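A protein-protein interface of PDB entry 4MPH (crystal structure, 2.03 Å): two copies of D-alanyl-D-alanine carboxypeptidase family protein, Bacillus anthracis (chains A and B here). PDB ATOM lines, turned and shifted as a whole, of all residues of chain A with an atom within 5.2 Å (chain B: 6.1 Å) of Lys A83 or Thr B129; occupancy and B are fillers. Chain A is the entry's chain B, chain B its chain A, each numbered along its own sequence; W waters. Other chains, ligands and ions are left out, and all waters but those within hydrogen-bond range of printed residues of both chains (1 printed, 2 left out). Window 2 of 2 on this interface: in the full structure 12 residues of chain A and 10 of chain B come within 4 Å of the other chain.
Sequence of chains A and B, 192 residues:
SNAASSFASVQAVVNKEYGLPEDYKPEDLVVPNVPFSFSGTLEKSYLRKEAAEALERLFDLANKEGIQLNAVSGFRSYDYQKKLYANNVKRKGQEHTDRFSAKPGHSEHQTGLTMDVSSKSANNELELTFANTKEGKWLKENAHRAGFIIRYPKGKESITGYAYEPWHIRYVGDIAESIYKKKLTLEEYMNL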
ATOM      1  N   ASP A  79      -5.368  27.133  14.310  1.00  0.00           N
ATOM      2  CA  ASP A  79      -4.324  26.676  15.235  1.00  0.00           C
ATOM      3  C   ASP A  79      -4.709  25.401  15.982  1.00  0.00           C
ATOM      4  O   ASP A  79      -3.866  24.537  16.225  1.00  0.00           O
ATOM      5  CB  ASP A  79      -3.944  27.781  16.223  1.00  0.00           C
ATOM      6  CG  ASP A  79      -3.411  29.033  15.534  1.00  0.00           C
ATOM      7  OD1 ASP A  79      -2.998  28.967  14.348  1.00  0.00           O
ATOM      8  OD2 ASP A  79      -3.421  30.100  16.187  1.00  0.00           O
ATOM      9  N   TYR A  80      -5.980  25.280  16.355  1.00  0.00           N
ATOM     10  CA  TYR A  80      -6.441  24.055  16.999  1.00  0.00           C
ATOM     11  C   TYR A  80      -6.318  22.896  16.023  1.00  0.00           C
ATOM     12  O   TYR A  80      -5.779  21.845  16.360  1.00  0.00           O
ATOM     13  CB  TYR A  80      -7.888  24.191  17.467  1.00  0.00           C
ATOM     14  CG  TYR A  80      -8.471  22.898  17.991  1.00  0.00           C
ATOM     15  CD1 TYR A  80      -8.336  22.545  19.329  1.00  0.00           C
ATOM     16  CD2 TYR A  80      -9.155  22.029  17.150  1.00  0.00           C
ATOM     17  CE1 TYR A  80      -8.871  21.359  19.818  1.00  0.00           C
ATOM     18  CE2 TYR A  80      -9.697  20.838  17.633  1.00  0.00           C
ATOM     19  CZ  TYR A  80      -9.547  20.509  18.961  1.00  0.00           C
ATOM     20  OH  TYR A  80     -10.088  19.331  19.428  1.00  0.00           O
ATOM     21  N   GLN A  81      -6.805  23.108  14.803  1.00  0.00           N
ATOM     22  CA  GLN A  81      -6.805  22.067  13.782  1.00  0.00           C
ATOM     23  C   GLN A  81      -5.385  21.603  13.476  1.00  0.00           C
ATOM     24  O   GLN A  81      -5.149  20.429  13.170  1.00  0.00           O
ATOM     25  CB  GLN A  81      -7.481  22.577  12.499  1.00  0.00           C
ATOM     26  CG  GLN A  81      -7.861  21.480  11.500  1.00  0.00           C
ATOM     27  CD  GLN A  81      -8.924  20.508  12.049  1.00  0.00           C
ATOM     28  OE1 GLN A  81      -9.831  20.901  12.791  1.00  0.00           O
ATOM     29  NE2 GLN A  81      -8.802  19.231  11.688  1.00  0.00           N
ATOM     30  N   LYS A  82      -4.435  22.523  13.587  1.00  0.00           N
ATOM     31  CA  LYS A  82      -3.051  22.224  13.234  1.00  0.00           C
ATOM     32  C   LYS A  82      -2.430  21.176  14.170  1.00  0.00           C
ATOM     33  O   LYS A  82      -1.720  20.273  13.725  1.00  0.00           O
ATOM     34  CB  LYS A  82      -2.220  23.509  13.196  1.00  0.00           C
ATOM     35  CG  LYS A  82      -0.756  23.292  12.833  1.00  0.00           C
ATOM     36  CD  LYS A  82      -0.082  24.593  12.428  1.00  0.00           C
ATOM     37  CE  LYS A  82       0.277  24.595  10.945  1.00  0.00           C
ATOM     38  NZ  LYS A  82       1.249  23.516  10.600  1.00  0.00           N
ATOM     39  N   LYS A  83      -2.730  21.282  15.458  1.00  0.00           N
ATOM     40  CA  LYS A  83      -2.190  20.347  16.436  1.00  0.00           C
ATOM     41  C   LYS A  83      -2.946  19.026  16.410  1.00  0.00           C
ATOM     42  O   LYS A  83      -2.361  17.956  16.608  1.00  0.00           O
ATOM     43  CB  LYS A  83      -2.253  20.956  17.834  1.00  0.00           C
ATOM     44  CG  LYS A  83      -1.604  22.322  17.941  1.00  0.00           C
ATOM     45  CD  LYS A  83      -1.878  22.947  19.300  1.00  0.00           C
ATOM     46  CE  LYS A  83      -1.205  24.305  19.420  1.00  0.00           C
ATOM     47  NZ  LYS A  83      -1.497  24.965  20.723  1.00  0.00           N
ATOM     48  N   LEU A  84      -4.251  19.103  16.178  1.00  0.00           N
ATOM     49  CA  LEU A  84      -5.069  17.900  16.071  1.00  0.00           C
ATOM     50  C   LEU A  84      -4.604  17.061  14.881  1.00  0.00           C
ATOM     51  O   LEU A  84      -4.529  15.835  14.964  1.00  0.00           O
ATOM     52  CB  LEU A  84      -6.548  18.258  15.917  1.00  0.00           C
ATOM     53  CG  LEU A  84      -7.520  17.083  16.068  1.00  0.00           C
ATOM     54  CD1 LEU A  84      -7.762  16.797  17.539  1.00  0.00           C
ATOM     55  CD2 LEU A  84      -8.833  17.335  15.331  1.00  0.00           C
ATOM     56  N   TYR A  85      -4.280  17.731  13.779  1.00  0.00           N
ATOM     57  CA  TYR A  85      -3.794  17.039  12.594  1.00  0.00           C
ATOM     58  C   TYR A  85      -2.438  16.395  12.857  1.00  0.00           C
ATOM     59  O   TYR A  85      -2.230  15.219  12.553  1.00  0.00           O
ATOM     60  CB  TYR A  85      -3.694  17.991  11.399  1.00  0.00           C
ATOM     61  CG  TYR A  85      -3.215  17.299  10.146  1.00  0.00           C
ATOM     62  CD1 TYR A  85      -4.073  16.489   9.407  1.00  0.00           C
ATOM     63  CD2 TYR A  85      -1.902  17.443   9.706  1.00  0.00           C
ATOM     64  CE1 TYR A  85      -3.638  15.845   8.262  1.00  0.00           C
ATOM     65  CE2 TYR A  85      -1.458  16.803   8.560  1.00  0.00           C
ATOM     66  CZ  TYR A  85      -2.329  16.004   7.842  1.00  0.00           C
ATOM     67  OH  TYR A  85      -1.892  15.367   6.702  1.00  0.00           O
ATOM     68  N   ALA A  86      -1.517  17.174  13.418  1.00  0.00           N
ATOM     69  CA  ALA A  86      -0.179  16.681  13.729  1.00  0.00           C
ATOM     70  C   ALA A  86      -0.199  15.508  14.719  1.00  0.00           C
ATOM     71  O   ALA A  86       0.526  14.526  14.546  1.00  0.00           O
ATOM     72  CB  ALA A  86       0.685  17.815  14.257  1.00  0.00           C
ATOM     73  N   ASN A  87      -1.033  15.609  15.751  1.00  0.00           N
ATOM     74  CA  ASN A  87      -1.091  14.584  16.795  1.00  0.00           C
ATOM     75  C   ASN A  87      -1.988  13.392  16.447  1.00  0.00           C
ATOM     76  O   ASN A  87      -2.242  12.529  17.291  1.00  0.00           O
ATOM     77  CB  ASN A  87      -1.514  15.201  18.134  1.00  0.00           C
ATOM     78  CG  ASN A  87      -0.456  16.128  18.712  1.00  0.00           C
ATOM     79  OD1 ASN A  87       0.743  15.951  18.477  1.00  0.00           O
ATOM     80  ND2 ASN A  87      -0.898  17.122  19.479  1.00  0.00           N
ATOM     81  N   ASN A  88      -2.471  13.359  15.209  1.00  0.00           N
ATOM     82  CA  ASN A  88      -3.240  12.222  14.712  1.00  0.00           C
ATOM     83  C   ASN A  88      -2.514  11.550  13.549  1.00  0.00           C
ATOM     84  O   ASN A  88      -2.908  10.476  13.088  1.00  0.00           O
ATOM     85  CB  ASN A  88      -4.654  12.649  14.298  1.00  0.00           C
ATOM     86  CG  ASN A  88      -5.529  13.032  15.490  1.00  0.00           C
ATOM     87  OD1 ASN A  88      -5.028  13.376  16.563  1.00  0.00           O
ATOM     88  ND2 ASN A  88      -6.843  12.973  15.300  1.00  0.00           N
ATOM     89  N   SER B 121      -7.289  25.059  29.567  1.00  0.00           N
ATOM     90  CA  SER B 121      -6.198  25.411  28.649  1.00  0.00           C
ATOM     91  C   SER B 121      -6.008  24.362  27.548  1.00  0.00           C
ATOM     92  O   SER B 121      -5.385  24.642  26.525  1.00  0.00           O
ATOM     93  CB  SER B 121      -4.883  25.586  29.415  1.00  0.00           C
ATOM     94  OG  SER B 121      -4.642  24.446  30.230  1.00  0.00           O
ATOM     95  N   ALA B 122      -6.536  23.156  27.761  1.00  0.00           N
ATOM     96  CA  ALA B 122      -6.481  22.105  26.743  1.00  0.00           C
ATOM     97  C   ALA B 122      -7.883  21.764  26.234  1.00  0.00           C
ATOM     98  O   ALA B 122      -8.116  20.650  25.737  1.00  0.00           O
ATOM     99  CB  ALA B 122      -5.810  20.858  27.306  1.00  0.00           C
ATOM    100  N   GLU B 125     -10.020  18.440  26.726  1.00  0.00           N
ATOM    101  CA  GLU B 125      -9.928  17.293  25.832  1.00  0.00           C
ATOM    102  C   GLU B 125      -8.750  16.388  26.182  1.00  0.00           C
ATOM    103  O   GLU B 125      -7.755  16.831  26.782  1.00  0.00           O
ATOM    104  CB  GLU B 125      -9.880  17.772  24.364  1.00  0.00           C
ATOM    105  CG  GLU B 125     -11.232  18.307  23.895  1.00  0.00           C
ATOM    106  CD  GLU B 125     -11.176  19.008  22.543  1.00  0.00           C
ATOM    107  OE1 GLU B 125     -10.093  19.030  21.914  1.00  0.00           O
ATOM    108  OE2 GLU B 125     -12.223  19.544  22.113  1.00  0.00           O
ATOM    109  N   GLU B 127      -6.014  15.018  24.827  1.00  0.00           N
ATOM    110  CA  GLU B 127      -5.118  15.076  23.680  1.00  0.00           C
ATOM    111  C   GLU B 127      -3.704  15.331  24.176  1.00  0.00           C
ATOM    112  O   GLU B 127      -3.502  15.701  25.339  1.00  0.00           O
ATOM    113  CB  GLU B 127      -5.545  16.187  22.713  1.00  0.00           C
ATOM    114  CG  GLU B 127      -6.934  16.006  22.095  1.00  0.00           C
ATOM    115  CD  GLU B 127      -6.983  14.916  21.032  1.00  0.00           C
ATOM    116  OE1 GLU B 127      -5.912  14.550  20.497  1.00  0.00           O
ATOM    117  OE2 GLU B 127      -8.096  14.428  20.723  1.00  0.00           O
ATOM    118  N   LEU B 128      -2.731  15.131  23.292  1.00  0.00           N
ATOM    119  CA  LEU B 128      -1.328  15.303  23.644  1.00  0.00           C
ATOM    120  C   LEU B 128      -1.007  16.735  24.044  1.00  0.00           C
ATOM    121  O   LEU B 128      -0.069  16.971  24.804  1.00  0.00           O
ATOM    122  CB  LEU B 128      -0.424  14.859  22.491  1.00  0.00           C
ATOM    123  CG  LEU B 128      -0.297  13.341  22.339  1.00  0.00           C
ATOM    124  CD1 LEU B 128       0.513  12.992  21.097  1.00  0.00           C
ATOM    125  CD2 LEU B 128       0.347  12.728  23.581  1.00  0.00           C
ATOM    126  N   THR B 129      -1.785  17.691  23.545  1.00  0.00           N
ATOM    127  CA  THR B 129      -1.557  19.094  23.896  1.00  0.00           C
ATOM    128  C   THR B 129      -1.654  19.336  25.410  1.00  0.00           C
ATOM    129  O   THR B 129      -1.041  20.263  25.938  1.00  0.00           O
ATOM    130  CB  THR B 129      -2.520  20.045  23.153  1.00  0.00           C
ATOM    131  OG1 THR B 129      -3.869  19.652  23.412  1.00  0.00           O
ATOM    132  CG2 THR B 129      -2.274  20.000  21.671  1.00  0.00           C
ATOM    133  N   PHE B 130      -2.411  18.503  26.114  1.00  0.00           N
ATOM    134  CA  PHE B 130      -2.531  18.663  27.559  1.00  0.00           C
ATOM    135  C   PHE B 130      -1.156  18.627  28.233  1.00  0.00           C
ATOM    136  O   PHE B 130      -0.916  19.316  29.230  1.00  0.00           O
ATOM    137  CB  PHE B 130      -3.453  17.581  28.139  1.00  0.00           C
ATOM    138  CG  PHE B 130      -3.583  17.624  29.641  1.00  0.00           C
ATOM    139  CD1 PHE B 130      -4.055  18.765  30.288  1.00  0.00           C
ATOM    140  CD2 PHE B 130      -3.265  16.503  30.411  1.00  0.00           C
ATOM    141  CE1 PHE B 130      -4.188  18.803  31.685  1.00  0.00           C
ATOM    142  CE2 PHE B 130      -3.392  16.525  31.813  1.00  0.00           C
ATOM    143  CZ  PHE B 130      -3.857  17.680  32.454  1.00  0.00           C
ATOM    144  N   ALA B 131      -0.243  17.844  27.667  1.00  0.00           N
ATOM    145  CA  ALA B 131       1.092  17.696  28.244  1.00  0.00           C
ATOM    146  C   ALA B 131       1.871  19.009  28.261  1.00  0.00           C
ATOM    147  O   ALA B 131       2.760  19.196  29.090  1.00  0.00           O
ATOM    148  CB  ALA B 131       1.882  16.635  27.496  1.00  0.00           C
ATOM    149  N   ASN B 132       1.560  19.912  27.337  1.00  0.00           N
ATOM    150  CA  ASN B 132       2.321  21.156  27.235  1.00  0.00           C
ATOM    151  C   ASN B 132       1.688  22.314  28.005  1.00  0.00           C
ATOM    152  O   ASN B 132       2.156  23.447  27.937  1.00  0.00           O
ATOM    153  CB  ASN B 132       2.525  21.536  25.763  1.00  0.00           C
ATOM    154  CG  ASN B 132       3.406  20.542  25.030  1.00  0.00           C
ATOM    155  OD1 ASN B 132       4.336  19.982  25.614  1.00  0.00           O
ATOM    156  ND2 ASN B 132       3.114  20.312  23.750  1.00  0.00           N
ATOM    157  N   THR B 133       0.619  22.031  28.737  1.00  0.00           N
ATOM    158  CA  THR B 133      -0.018  23.058  29.549  1.00  0.00           C
ATOM    159  C   THR B 133       0.618  23.049  30.934  1.00  0.00           C
ATOM    160  O   THR B 133       1.204  22.040  31.345  1.00  0.00           O
ATOM    161  CB  THR B 133      -1.532  22.808  29.686  1.00  0.00           C
ATOM    162  OG1 THR B 133      -1.744  21.576  30.386  1.00  0.00           O
ATOM    163  CG2 THR B 133      -2.194  22.732  28.308  1.00  0.00           C
ATOM    164  N   PRO B 166      -0.890  11.754  28.720  1.00  0.00           N
ATOM    165  CA  PRO B 166      -0.672  12.644  29.872  1.00  0.00           C
ATOM    166  C   PRO B 166      -1.939  12.949  30.664  1.00  0.00           C
ATOM    167  O   PRO B 166      -1.832  13.518  31.760  1.00  0.00           O
ATOM    168  CB  PRO B 166      -0.122  13.929  29.238  1.00  0.00           C
ATOM    169  CG  PRO B 166      -0.618  13.887  27.779  1.00  0.00           C
ATOM    170  CD  PRO B 166      -0.625  12.421  27.427  1.00  0.00           C
HETATM  171  O   HOH W   1      -8.013  12.666  18.349  1.00  0.00           O
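OE1 of Glu B125 is in hydrogen-bond range of OH of Tyr A80 (2.5 Å).
Water W1 bridges the side-chain carboxylate (OE2) of Glu B127 and the side-chain amide nitrogen (ND2) of Asn A88.
No position is printed for both chains. Of the 5 pairs that touch across the chains among the printed residues, none has its exchanged pair printed and touching as well.
Of the printed residues of chain B, Tyr A80 touches Glu B125 (2.5 Å). Lys A83 touches one residue of chain B. Printed residues of chain B within 4 Å of Asn A87: Leu B128 and Thr B129. Asn A88 touches none of the printed residues of chain B. Of the printed residues of chain A, Glu B127 touches Leu A84 (3.98 Å). Thr B129 touches two residues of chain A. The nearest printed residue of chain A that does not touch Thr B129 is Leu A84 (5.9 Å).
Among the printed residues, pairs that only touch across the chains: Asn A87 with Leu B128 (3.8 Å), Lys A83 with Thr B129 (3.8 Å), Asn A87 with Thr B129 (3.9 Å) and Leu A84 with Glu B127 (3.98 Å).
The side-chain amide nitrogen of Asn A87 lies close to the backbone carbonyl oxygen of Lys A83 (3.3 Å). The side-chain amide oxygen (OD1) of Asn A88 lies close to the backbone carbonyl oxygen (O) of Leu A84 (3.0 Å).
Printed residues of chain A that touch a printed residue of chain B: Tyr A80, Lys A83, Leu A84 and Asn A87. Hydrophobic or aromatic side chains of chain A that line the printed part of chain B: Tyr A80 and Leu A84. Of the 11 printed residues of chain B, 4 touch a printed residue of chain A. Among the printed residues, no Asp or Glu carboxylate lies within 4 Å of a Lys or Arg side-chain nitrogen of the other chain.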
